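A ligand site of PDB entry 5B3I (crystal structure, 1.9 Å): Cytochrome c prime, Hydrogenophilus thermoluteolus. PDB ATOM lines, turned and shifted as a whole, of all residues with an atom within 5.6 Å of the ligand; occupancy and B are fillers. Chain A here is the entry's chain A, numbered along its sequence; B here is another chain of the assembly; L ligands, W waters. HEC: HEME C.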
ATOM      1  N   VAL A   9       2.087 -11.631 -20.036  1.00  0.00           N
ATOM      2  CA  VAL A   9       1.870 -10.186 -20.039  1.00  0.00           C
ATOM      3  C   VAL A   9       3.193  -9.450 -19.886  1.00  0.00           C
ATOM      4  O   VAL A   9       3.483  -8.502 -20.618  1.00  0.00           O
ATOM      5  CB  VAL A   9       0.902  -9.773 -18.921  1.00  0.00           C
ATOM      6  CG1 VAL A   9       0.750  -8.263 -18.868  1.00  0.00           C
ATOM      7  CG2 VAL A   9      -0.417 -10.436 -19.126  1.00  0.00           C
ATOM      8  N   ARG A  12       5.264  -9.713 -23.083  1.00  0.00           N
ATOM      9  CA  ARG A  12       4.805  -8.907 -24.209  1.00  0.00           C
ATOM     10  C   ARG A  12       5.002  -7.410 -23.913  1.00  0.00           C
ATOM     11  O   ARG A  12       5.402  -6.670 -24.796  1.00  0.00           O
ATOM     12  CB  ARG A  12       3.353  -9.206 -24.583  1.00  0.00           C
ATOM     13  CG  ARG A  12       2.252  -8.720 -23.665  1.00  0.00           C
ATOM     14  CD  ARG A  12       0.979  -9.494 -24.030  1.00  0.00           C
ATOM     15  NE  ARG A  12      -0.192  -9.076 -23.296  1.00  0.00           N
ATOM     16  CZ  ARG A  12      -1.239  -9.855 -23.003  1.00  0.00           C
ATOM     17  NH1 ARG A  12      -1.282 -11.138 -23.355  1.00  0.00           N
ATOM     18  NH2 ARG A  12      -2.254  -9.348 -22.337  1.00  0.00           N
ATOM     19  N   GLN A  13       4.729  -6.978 -22.686  1.00  0.00           N
ATOM     20  CA  GLN A  13       5.008  -5.606 -22.300  1.00  0.00           C
ATOM     21  C   GLN A  13       6.499  -5.278 -22.471  1.00  0.00           C
ATOM     22  O   GLN A  13       6.857  -4.197 -22.958  1.00  0.00           O
ATOM     23  CB  GLN A  13       4.554  -5.333 -20.867  1.00  0.00           C
ATOM     24  CG  GLN A  13       3.032  -5.331 -20.709  1.00  0.00           C
ATOM     25  CD  GLN A  13       2.591  -5.184 -19.259  1.00  0.00           C
ATOM     26  OE1 GLN A  13       3.375  -5.416 -18.329  1.00  0.00           O
ATOM     27  NE2 GLN A  13       1.326  -4.811 -19.065  1.00  0.00           N
ATOM     28  N   ALA A  14       7.365  -6.201 -22.061  1.00  0.00           N
ATOM     29  CA  ALA A  14       8.800  -6.007 -22.233  1.00  0.00           C
ATOM     30  C   ALA A  14       9.157  -5.871 -23.698  1.00  0.00           C
ATOM     31  O   ALA A  14       9.947  -5.001 -24.070  1.00  0.00           O
ATOM     32  CB  ALA A  14       9.567  -7.169 -21.627  1.00  0.00           C
ATOM     33  N   TYR A  16       7.269  -4.783 -26.224  1.00  0.00           N
ATOM     34  CA  TYR A  16       6.848  -3.546 -26.823  1.00  0.00           C
ATOM     35  C   TYR A  16       7.766  -2.416 -26.392  1.00  0.00           C
ATOM     36  O   TYR A  16       8.140  -1.616 -27.166  1.00  0.00           O
ATOM     37  CB  TYR A  16       5.386  -3.221 -26.571  1.00  0.00           C
ATOM     38  CG  TYR A  16       4.429  -4.196 -27.201  1.00  0.00           C
ATOM     39  CD1 TYR A  16       4.184  -4.201 -28.547  1.00  0.00           C
ATOM     40  CD2 TYR A  16       3.788  -5.104 -26.473  1.00  0.00           C
ATOM     41  CE1 TYR A  16       3.284  -5.063 -29.108  1.00  0.00           C
ATOM     42  CE2 TYR A  16       2.907  -6.003 -27.032  1.00  0.00           C
ATOM     43  CZ  TYR A  16       2.678  -5.993 -28.368  1.00  0.00           C
ATOM     44  OH  TYR A  16       1.840  -6.889 -28.925  1.00  0.00           O
ATOM     45  N   THR A  17       8.087  -2.400 -25.113  1.00  0.00           N
ATOM     46  CA  THR A  17       8.854  -1.294 -24.547  1.00  0.00           C
ATOM     47  C   THR A  17      10.262  -1.281 -25.128  1.00  0.00           C
ATOM     48  O   THR A  17      10.831  -0.208 -25.331  1.00  0.00           O
ATOM     49  CB  THR A  17       8.849  -1.364 -23.011  1.00  0.00           C
ATOM     50  OG1 THR A  17       7.552  -0.921 -22.571  1.00  0.00           O
ATOM     51  CG2 THR A  17       9.873  -0.457 -22.419  1.00  0.00           C
ATOM     52  N   MET A  19      10.956  -2.278 -28.242  1.00  0.00           N
ATOM     53  CA  MET A  19      10.793  -1.630 -29.541  1.00  0.00           C
ATOM     54  C   MET A  19      10.646  -0.114 -29.374  1.00  0.00           C
ATOM     55  O   MET A  19      11.183   0.666 -30.168  1.00  0.00           O
ATOM     56  CB  MET A  19       9.574  -2.193 -30.287  1.00  0.00           C
ATOM     57  CG  MET A  19       9.762  -3.629 -30.835  1.00  0.00           C
ATOM     58  SD  MET A  19       8.559  -4.147 -32.066  1.00  0.00           S
ATOM     59  CE  MET A  19       7.085  -4.154 -31.028  1.00  0.00           C
ATOM     60  N   ALA A  20       9.940   0.306 -28.326  1.00  0.00           N
ATOM     61  CA  ALA A  20       9.761   1.739 -28.093  1.00  0.00           C
ATOM     62  C   ALA A  20      11.097   2.436 -27.868  1.00  0.00           C
ATOM     63  O   ALA A  20      11.316   3.504 -28.418  1.00  0.00           O
ATOM     64  CB  ALA A  20       8.827   1.976 -26.930  1.00  0.00           C
ATOM     65  N   MET A  23      12.777   2.648 -31.381  1.00  0.00           N
ATOM     66  CA  MET A  23      12.095   3.625 -32.200  1.00  0.00           C
ATOM     67  C   MET A  23      12.528   5.016 -31.763  1.00  0.00           C
ATOM     68  O   MET A  23      12.776   5.881 -32.595  1.00  0.00           O
ATOM     69  CB  MET A  23      10.568   3.507 -32.090  1.00  0.00           C
ATOM     70  CG  MET A  23      10.012   2.236 -32.741  1.00  0.00           C
ATOM     71  SD  MET A  23       9.928   2.274 -34.541  1.00  0.00           S
ATOM     72  CE  MET A  23       8.511   3.321 -34.791  1.00  0.00           C
ATOM     73  N   ILE A  49      13.816  -3.903 -33.884  1.00  0.00           N
ATOM     74  CA  ILE A  49      12.393  -3.754 -34.152  1.00  0.00           C
ATOM     75  C   ILE A  49      11.895  -4.844 -35.116  1.00  0.00           C
ATOM     76  O   ILE A  49      10.876  -5.482 -34.865  1.00  0.00           O
ATOM     77  CB  ILE A  49      12.090  -2.348 -34.714  1.00  0.00           C
ATOM     78  CG1 ILE A  49      12.397  -1.292 -33.632  1.00  0.00           C
ATOM     79  CG2 ILE A  49      10.633  -2.290 -35.155  1.00  0.00           C
ATOM     80  CD1 ILE A  49      12.683   0.091 -34.174  1.00  0.00           C
ATOM     81  N   TYR A  61      -0.522 -14.278 -26.422  1.00  0.00           N
ATOM     82  CA  TYR A  61      -1.908 -13.806 -26.294  1.00  0.00           C
ATOM     83  C   TYR A  61      -2.927 -14.953 -26.101  1.00  0.00           C
ATOM     84  O   TYR A  61      -3.154 -15.800 -26.999  1.00  0.00           O
ATOM     85  CB  TYR A  61      -2.297 -12.962 -27.527  1.00  0.00           C
ATOM     86  CG  TYR A  61      -1.694 -11.561 -27.521  1.00  0.00           C
ATOM     87  CD1 TYR A  61      -2.305 -10.530 -26.833  1.00  0.00           C
ATOM     88  CD2 TYR A  61      -0.509 -11.295 -28.204  1.00  0.00           C
ATOM     89  CE1 TYR A  61      -1.759  -9.265 -26.813  1.00  0.00           C
ATOM     90  CE2 TYR A  61       0.043 -10.027 -28.191  1.00  0.00           C
ATOM     91  CZ  TYR A  61      -0.585  -9.012 -27.500  1.00  0.00           C
ATOM     92  OH  TYR A  61      -0.029  -7.753 -27.488  1.00  0.00           O
ATOM     93  N   LYS A  72       2.722  -4.220 -15.261  1.00  0.00           N
ATOM     94  CA  LYS A  72       1.563  -3.453 -14.795  1.00  0.00           C
ATOM     95  C   LYS A  72       0.357  -4.172 -15.385  1.00  0.00           C
ATOM     96  O   LYS A  72       0.512  -5.043 -16.254  1.00  0.00           O
ATOM     97  CB  LYS A  72       1.644  -1.978 -15.235  1.00  0.00           C
ATOM     98  CG  LYS A  72       1.369  -1.765 -16.756  1.00  0.00           C
ATOM     99  CD  LYS A  72       1.746  -0.348 -17.262  1.00  0.00           C
ATOM    100  CE  LYS A  72       1.476  -0.230 -18.776  1.00  0.00           C
ATOM    101  NZ  LYS A  72       2.095   0.959 -19.518  1.00  0.00           N
ATOM    102  N   LYS A  73      -0.819  -3.826 -14.892  1.00  0.00           N
ATOM    103  CA  LYS A  73      -2.056  -4.391 -15.380  1.00  0.00           C
ATOM    104  C   LYS A  73      -2.103  -4.279 -16.889  1.00  0.00           C
ATOM    105  O   LYS A  73      -1.841  -3.208 -17.437  1.00  0.00           O
ATOM    106  CB  LYS A  73      -3.251  -3.671 -14.743  1.00  0.00           C
ATOM    107  CG  LYS A  73      -4.595  -4.293 -15.064  1.00  0.00           C
ATOM    108  CD  LYS A  73      -5.652  -3.764 -14.124  1.00  0.00           C
ATOM    109  CE  LYS A  73      -7.014  -4.352 -14.433  1.00  0.00           C
ATOM    110  NZ  LYS A  73      -8.023  -3.962 -13.384  1.00  0.00           N
ATOM    111  N   SER A  74      -2.385  -5.400 -17.544  1.00  0.00           N
ATOM    112  CA  SER A  74      -2.398  -5.466 -18.994  1.00  0.00           C
ATOM    113  C   SER A  74      -3.404  -4.474 -19.583  1.00  0.00           C
ATOM    114  O   SER A  74      -4.520  -4.336 -19.064  1.00  0.00           O
ATOM    115  CB  SER A  74      -2.736  -6.861 -19.486  1.00  0.00           C
ATOM    116  OG  SER A  74      -2.772  -6.909 -20.890  1.00  0.00           O
ATOM    117  N   ARG A  75      -2.982  -3.767 -20.628  1.00  0.00           N
ATOM    118  CA  ARG A  75      -3.823  -2.803 -21.332  1.00  0.00           C
ATOM    119  C   ARG A  75      -4.435  -3.408 -22.604  1.00  0.00           C
ATOM    120  O   ARG A  75      -4.971  -2.688 -23.451  1.00  0.00           O
ATOM    121  CB  ARG A  75      -2.995  -1.564 -21.624  1.00  0.00           C
ATOM    122  CG  ARG A  75      -2.510  -0.885 -20.330  1.00  0.00           C
ATOM    123  CD  ARG A  75      -1.438   0.121 -20.673  1.00  0.00           C
ATOM    124  NE  ARG A  75      -1.893   1.079 -21.674  1.00  0.00           N
ATOM    125  CZ  ARG A  75      -1.090   1.780 -22.451  1.00  0.00           C
ATOM    126  NH1 ARG A  75       0.233   1.600 -22.399  1.00  0.00           N
ATOM    127  NH2 ARG A  75      -1.602   2.629 -23.336  1.00  0.00           N
ATOM    128  N   LEU A  76      -4.334  -4.733 -22.729  1.00  0.00           N
ATOM    129  CA  LEU A  76      -4.951  -5.435 -23.851  1.00  0.00           C
ATOM    130  C   LEU A  76      -6.475  -5.287 -23.749  1.00  0.00           C
ATOM    131  O   LEU A  76      -7.070  -5.542 -22.689  1.00  0.00           O
ATOM    132  CB  LEU A  76      -4.566  -6.924 -23.843  1.00  0.00           C
ATOM    133  CG  LEU A  76      -5.217  -7.766 -24.945  1.00  0.00           C
ATOM    134  CD1 LEU A  76      -4.670  -7.340 -26.331  1.00  0.00           C
ATOM    135  CD2 LEU A  76      -5.076  -9.310 -24.716  1.00  0.00           C
ATOM    136  N   VAL A  87      -6.441  -8.663 -36.646  1.00  0.00           N
ATOM    137  CA  VAL A  87      -5.146  -8.801 -36.001  1.00  0.00           C
ATOM    138  C   VAL A  87      -4.062  -9.335 -36.991  1.00  0.00           C
ATOM    139  O   VAL A  87      -2.955  -8.815 -37.051  1.00  0.00           O
ATOM    140  CB  VAL A  87      -5.243  -9.681 -34.752  1.00  0.00           C
ATOM    141  CG1 VAL A  87      -3.890  -9.880 -34.150  1.00  0.00           C
ATOM    142  CG2 VAL A  87      -6.155  -9.015 -33.729  1.00  0.00           C
ATOM    143  N   ILE A  90      -3.103  -6.499 -39.450  1.00  0.00           N
ATOM    144  CA  ILE A  90      -2.275  -5.490 -38.818  1.00  0.00           C
ATOM    145  C   ILE A  90      -0.882  -6.045 -38.515  1.00  0.00           C
ATOM    146  O   ILE A  90       0.122  -5.380 -38.769  1.00  0.00           O
ATOM    147  CB  ILE A  90      -2.980  -4.987 -37.543  1.00  0.00           C
ATOM    148  CG1 ILE A  90      -4.240  -4.207 -37.951  1.00  0.00           C
ATOM    149  CG2 ILE A  90      -2.058  -4.153 -36.678  1.00  0.00           C
ATOM    150  CD1 ILE A  90      -5.156  -3.857 -36.791  1.00  0.00           C
ATOM    151  N   ALA A  91      -0.806  -7.235 -37.953  1.00  0.00           N
ATOM    152  CA  ALA A  91       0.486  -7.859 -37.606  1.00  0.00           C
ATOM    153  C   ALA A  91       1.382  -8.100 -38.828  1.00  0.00           C
ATOM    154  O   ALA A  91       2.576  -7.819 -38.801  1.00  0.00           O
ATOM    155  CB  ALA A  91       0.270  -9.152 -36.883  1.00  0.00           C
ATOM    156  N   PHE A  94       2.608  -4.943 -40.027  1.00  0.00           N
ATOM    157  CA  PHE A  94       3.705  -4.501 -39.146  1.00  0.00           C
ATOM    158  C   PHE A  94       5.035  -5.200 -39.504  1.00  0.00           C
ATOM    159  O   PHE A  94       6.067  -4.551 -39.660  1.00  0.00           O
ATOM    160  CB  PHE A  94       3.350  -4.724 -37.659  1.00  0.00           C
ATOM    161  CG  PHE A  94       4.449  -4.336 -36.694  1.00  0.00           C
ATOM    162  CD1 PHE A  94       5.073  -3.103 -36.792  1.00  0.00           C
ATOM    163  CD2 PHE A  94       4.847  -5.210 -35.666  1.00  0.00           C
ATOM    164  CE1 PHE A  94       6.089  -2.739 -35.912  1.00  0.00           C
ATOM    165  CE2 PHE A  94       5.853  -4.859 -34.788  1.00  0.00           C
ATOM    166  CZ  PHE A  94       6.475  -3.612 -34.913  1.00  0.00           C
ATOM    167  N   VAL A 120       6.446   2.518 -40.279  1.00  0.00           N
ATOM    168  CA  VAL A 120       6.447   1.647 -39.105  1.00  0.00           C
ATOM    169  C   VAL A 120       5.611   2.315 -38.001  1.00  0.00           C
ATOM    170  O   VAL A 120       4.746   1.662 -37.390  1.00  0.00           O
ATOM    171  CB  VAL A 120       7.857   1.334 -38.606  1.00  0.00           C
ATOM    172  CG1 VAL A 120       7.818   0.585 -37.263  1.00  0.00           C
ATOM    173  CG2 VAL A 120       8.580   0.464 -39.651  1.00  0.00           C
ATOM    174  N   ALA A 123       1.974   1.637 -38.309  1.00  0.00           N
ATOM    175  CA  ALA A 123       1.663   0.267 -37.988  1.00  0.00           C
ATOM    176  C   ALA A 123       1.559   0.084 -36.459  1.00  0.00           C
ATOM    177  O   ALA A 123       0.646  -0.617 -35.985  1.00  0.00           O
ATOM    178  CB  ALA A 123       2.708  -0.655 -38.575  1.00  0.00           C
ATOM    179  N   CYS A 124       2.472   0.676 -35.689  1.00  0.00           N
ATOM    180  CA  CYS A 124       2.339   0.630 -34.218  1.00  0.00           C
ATOM    181  C   CYS A 124       0.975   1.148 -33.782  1.00  0.00           C
ATOM    182  O   CYS A 124       0.297   0.478 -33.025  1.00  0.00           O
ATOM    183  CB  CYS A 124       3.429   1.449 -33.472  1.00  0.00           C
ATOM    184  SG  CYS A 124       5.179   1.107 -33.934  1.00  0.00           S
ATOM    185  N   CYS A 127      -2.431  -0.868 -34.501  1.00  0.00           N
ATOM    186  CA  CYS A 127      -2.754  -1.914 -33.527  1.00  0.00           C
ATOM    187  C   CYS A 127      -3.255  -1.333 -32.212  1.00  0.00           C
ATOM    188  O   CYS A 127      -4.291  -1.761 -31.693  1.00  0.00           O
ATOM    189  CB  CYS A 127      -1.547  -2.826 -33.270  1.00  0.00           C
ATOM    190  SG  CYS A 127      -1.991  -4.258 -32.303  1.00  0.00           S
ATOM    191  N   HIS A 128      -2.561  -0.315 -31.705  1.00  0.00           N
ATOM    192  CA  HIS A 128      -2.951   0.331 -30.455  1.00  0.00           C
ATOM    193  C   HIS A 128      -4.368   0.906 -30.513  1.00  0.00           C
ATOM    194  O   HIS A 128      -5.117   0.818 -29.553  1.00  0.00           O
ATOM    195  CB  HIS A 128      -1.962   1.461 -30.086  1.00  0.00           C
ATOM    196  CG  HIS A 128      -0.571   0.978 -29.843  1.00  0.00           C
ATOM    197  ND1 HIS A 128       0.540   1.786 -29.915  1.00  0.00           N
ATOM    198  CD2 HIS A 128      -0.115  -0.261 -29.515  1.00  0.00           C
ATOM    199  CE1 HIS A 128       1.612   1.074 -29.644  1.00  0.00           C
ATOM    200  NE2 HIS A 128       1.249  -0.174 -29.398  1.00  0.00           N
ATOM    201  N   PHE A 131      -6.626  -2.166 -30.118  1.00  0.00           N
ATOM    202  CA  PHE A 131      -6.443  -3.229 -29.119  1.00  0.00           C
ATOM    203  C   PHE A 131      -5.684  -2.844 -27.842  1.00  0.00           C
ATOM    204  O   PHE A 131      -5.452  -3.709 -27.004  1.00  0.00           O
ATOM    205  CB  PHE A 131      -5.750  -4.416 -29.793  1.00  0.00           C
ATOM    206  CG  PHE A 131      -6.470  -4.891 -31.025  1.00  0.00           C
ATOM    207  CD1 PHE A 131      -7.807  -5.262 -30.956  1.00  0.00           C
ATOM    208  CD2 PHE A 131      -5.837  -4.971 -32.237  1.00  0.00           C
ATOM    209  CE1 PHE A 131      -8.487  -5.676 -32.086  1.00  0.00           C
ATOM    210  CE2 PHE A 131      -6.515  -5.417 -33.364  1.00  0.00           C
ATOM    211  CZ  PHE A 131      -7.838  -5.764 -33.284  1.00  0.00           C
ATOM    212  N   ARG A 132      -5.285  -1.590 -27.692  1.00  0.00           N
ATOM    213  CA  ARG A 132      -4.564  -1.186 -26.478  1.00  0.00           C
ATOM    214  C   ARG A 132      -5.283  -0.041 -25.789  1.00  0.00           C
ATOM    215  O   ARG A 132      -5.495   0.998 -26.399  1.00  0.00           O
ATOM    216  CB  ARG A 132      -3.131  -0.747 -26.812  1.00  0.00           C
ATOM    217  CG  ARG A 132      -2.305  -0.431 -25.573  1.00  0.00           C
ATOM    218  CD  ARG A 132      -0.921   0.136 -25.867  1.00  0.00           C
ATOM    219  NE  ARG A 132      -0.983   1.526 -26.318  1.00  0.00           N
ATOM    220  CZ  ARG A 132       0.072   2.305 -26.525  1.00  0.00           C
ATOM    221  NH1 ARG A 132       1.297   1.837 -26.298  1.00  0.00           N
ATOM    222  NH2 ARG A 132      -0.092   3.552 -26.936  1.00  0.00           N
ATOM    223  N   PHE B  71      10.588  -0.685 -14.057  1.00  0.00           N
ATOM    224  CA  PHE B  71       9.411  -1.495 -13.687  1.00  0.00           C
ATOM    225  C   PHE B  71       9.573  -1.881 -12.232  1.00  0.00           C
ATOM    226  O   PHE B  71       8.595  -2.057 -11.514  1.00  0.00           O
ATOM    227  CB  PHE B  71       9.282  -2.728 -14.556  1.00  0.00           C
ATOM    228  CG  PHE B  71       8.942  -2.425 -15.965  1.00  0.00           C
ATOM    229  CD1 PHE B  71       7.804  -1.705 -16.286  1.00  0.00           C
ATOM    230  CD2 PHE B  71       9.774  -2.852 -16.989  1.00  0.00           C
ATOM    231  CE1 PHE B  71       7.488  -1.426 -17.619  1.00  0.00           C
ATOM    232  CE2 PHE B  71       9.468  -2.582 -18.316  1.00  0.00           C
ATOM    233  CZ  PHE B  71       8.326  -1.872 -18.645  1.00  0.00           C
HETATM  234 FE   HEC L   1       2.413  -1.923 -28.786  1.00  0.00          FE
HETATM  235  CHA HEC L   1       1.789  -1.949 -25.393  1.00  0.00           C
HETATM  236  CHB HEC L   1       5.034   0.395 -28.179  1.00  0.00           C
HETATM  237  CHC HEC L   1       3.454  -2.129 -32.089  1.00  0.00           C
HETATM  238  CHD HEC L   1      -0.111  -3.980 -29.379  1.00  0.00           C
HETATM  239  NA  HEC L   1       3.167  -0.927 -27.221  1.00  0.00           N
HETATM  240  C1A HEC L   1       2.807  -1.171 -25.887  1.00  0.00           C
HETATM  241  C2A HEC L   1       3.688  -0.495 -25.034  1.00  0.00           C
HETATM  242  C3A HEC L   1       4.599   0.143 -25.803  1.00  0.00           C
HETATM  243  C4A HEC L   1       4.272  -0.088 -27.144  1.00  0.00           C
HETATM  244  CMA HEC L   1       5.732   0.997 -25.273  1.00  0.00           C
HETATM  245  CAA HEC L   1       3.677  -0.488 -23.529  1.00  0.00           C
HETATM  246  CBA HEC L   1       4.215  -1.810 -22.969  1.00  0.00           C
HETATM  247  CGA HEC L   1       4.455  -1.702 -21.470  1.00  0.00           C
HETATM  248  O1A HEC L   1       3.530  -1.855 -20.654  1.00  0.00           O
HETATM  249  O2A HEC L   1       5.591  -1.424 -21.044  1.00  0.00           O
HETATM  250  NB  HEC L   1       3.992  -1.041 -29.878  1.00  0.00           N
HETATM  251  C1B HEC L   1       4.894  -0.124 -29.474  1.00  0.00           C
HETATM  252  C2B HEC L   1       5.745   0.246 -30.559  1.00  0.00           C
HETATM  253  C3B HEC L   1       5.310  -0.422 -31.670  1.00  0.00           C
HETATM  254  C4B HEC L   1       4.157  -1.259 -31.211  1.00  0.00           C
HETATM  255  CMB HEC L   1       6.878   1.241 -30.486  1.00  0.00           C
HETATM  256  CAB HEC L   1       5.844  -0.328 -33.058  1.00  0.00           C
HETATM  257  CBB HEC L   1       7.152  -0.531 -33.311  1.00  0.00           C
HETATM  258  NC  HEC L   1       1.769  -2.905 -30.504  1.00  0.00           N
HETATM  259  C1C HEC L   1       2.349  -2.904 -31.733  1.00  0.00           C
HETATM  260  C2C HEC L   1       1.609  -3.761 -32.568  1.00  0.00           C
HETATM  261  C3C HEC L   1       0.579  -4.318 -31.810  1.00  0.00           C
HETATM  262  C4C HEC L   1       0.688  -3.748 -30.494  1.00  0.00           C
HETATM  263  CMC HEC L   1       1.938  -4.024 -34.039  1.00  0.00           C
HETATM  264  CAC HEC L   1      -0.494  -5.268 -32.275  1.00  0.00           C
HETATM  265  CBC HEC L   1      -0.263  -6.240 -33.158  1.00  0.00           C
HETATM  266  ND  HEC L   1       1.168  -2.755 -27.620  1.00  0.00           N
HETATM  267  C1D HEC L   1       0.185  -3.565 -28.060  1.00  0.00           C
HETATM  268  C2D HEC L   1      -0.639  -4.040 -26.919  1.00  0.00           C
HETATM  269  C3D HEC L   1      -0.100  -3.499 -25.803  1.00  0.00           C
HETATM  270  C4D HEC L   1       1.023  -2.681 -26.273  1.00  0.00           C
HETATM  271  CMD HEC L   1      -1.810  -4.986 -26.978  1.00  0.00           C
HETATM  272  CAD HEC L   1      -0.574  -3.708 -24.374  1.00  0.00           C
HETATM  273  CBD HEC L   1       0.120  -4.978 -23.836  1.00  0.00           C
HETATM  274  CGD HEC L   1      -0.236  -5.310 -22.402  1.00  0.00           C
HETATM  275  O1D HEC L   1      -0.251  -4.424 -21.484  1.00  0.00           O
HETATM  276  O2D HEC L   1      -0.535  -6.511 -22.125  1.00  0.00           O
HETATM  277  O   HOH W   1       4.415  -2.155 -18.335  1.00  0.00           O
HETATM  278  O   HOH W   2       1.013  -2.026 -21.833  1.00  0.00           O
HETATM  279  O   HOH W   3       2.321  -7.553 -31.521  1.00  0.00           O
HETATM  280  O   HOH W   4       5.336   0.932 -19.417  1.00  0.00           O
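FE of the ligand is bound by NE2 of His 128 (2.2 Å).
The side-chain amino group (NZ) of Lys 72 is in salt-bridge range of an oxygen (O1A) of the ligand (3.4 Å).
The side-chain hydroxyl (OG1) of Thr 17 lies within hydrogen-bond range of an oxygen (O2A) of the ligand.
The side-chain amide nitrogen (NE2) of Gln 13 lies within hydrogen-bond range of an oxygen (O1D) of the ligand (2.9 Å).
NE of Arg 12 lies within salt-bridge range of O2D of the ligand, at 2.8 Å.
SG of Cys 124 is covalently linked to CAB of the ligand.
A carbon (CAC) of the ligand is covalently linked to the side-chain sulfur (SG) of Cys 127, at 1.8 Å.
The backbone NH of Arg 75 lies within hydrogen-bond range of an oxygen (O1D) of the ligand (2.9 Å).
The side-chain hydroxyl (OG) of Ser 74 lies within hydrogen-bond range of an oxygen (O2D) of the ligand (2.6 Å).
The side-chain hydroxyl of Tyr 16 is in hydrogen-bond range of the side-chain hydroxyl of Tyr 61 (2.5 Å).
OG1 of Thr 17 is in hydrogen-bond range of O of Gln 13 (3.4 Å).
OG of Ser 74 lies within hydrogen-bond range of NH2 of Arg 12 (2.9 Å).
NE2 of Gln 13 sits at hydrogen-bond distance from O of Lys 72.
A ring nitrogen (ND1) of His 128 sits close to the backbone carbonyl oxygen (O) of Cys 124 (3.4 Å).
OG of Ser 74 sits at hydrogen-bond distance from N of Leu 76, 3.2 Å away.
NH1 of Arg 132 lies close to NA of the ligand (3.5 Å).
Val 9 touches the ligand.
Tyr 16 touches the ligand (CD1 to FE, 2.9 Å).
Ala 20 touches the ligand (CB to CMA, 3.6 Å).
Met 23 touches the ligand (CG to CMB, 3.99 Å).
OH of Tyr 61 touches CMD of the ligand, at 3.3 Å.
Leu 76 touches the ligand (CD1 to CMD, 3.8 Å).
CD2 of Phe 94 touches CMC of the ligand, at 3.5 Å.
O of Phe 131 touches CMD of the ligand, at 3.9 Å.
Phe 71 of chain B touches the ligand (CZ to O2A, 3.7 Å).
Within 4 Å of the ligand: Val 9, Arg 12, Gln 13, Tyr 16, Thr 17, Ala 20, Met 23, Tyr 61, Lys 72, Ser 74, Arg 75, Leu 76, Phe 94, Cys 124, Cys 127, His 128, Phe 131, Arg 132 and Phe 71 of chain B.
The nearest printed residue that does not touch the ligand is Met 19 (4.1 Å).
Water W1 bridges O1A of the ligand (2.5 Å) and OE1 of Gln 13 (3.4 Å).
Water W4 bridges an oxygen (O2A) of the ligand and the side-chain amino group of Lys 72.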
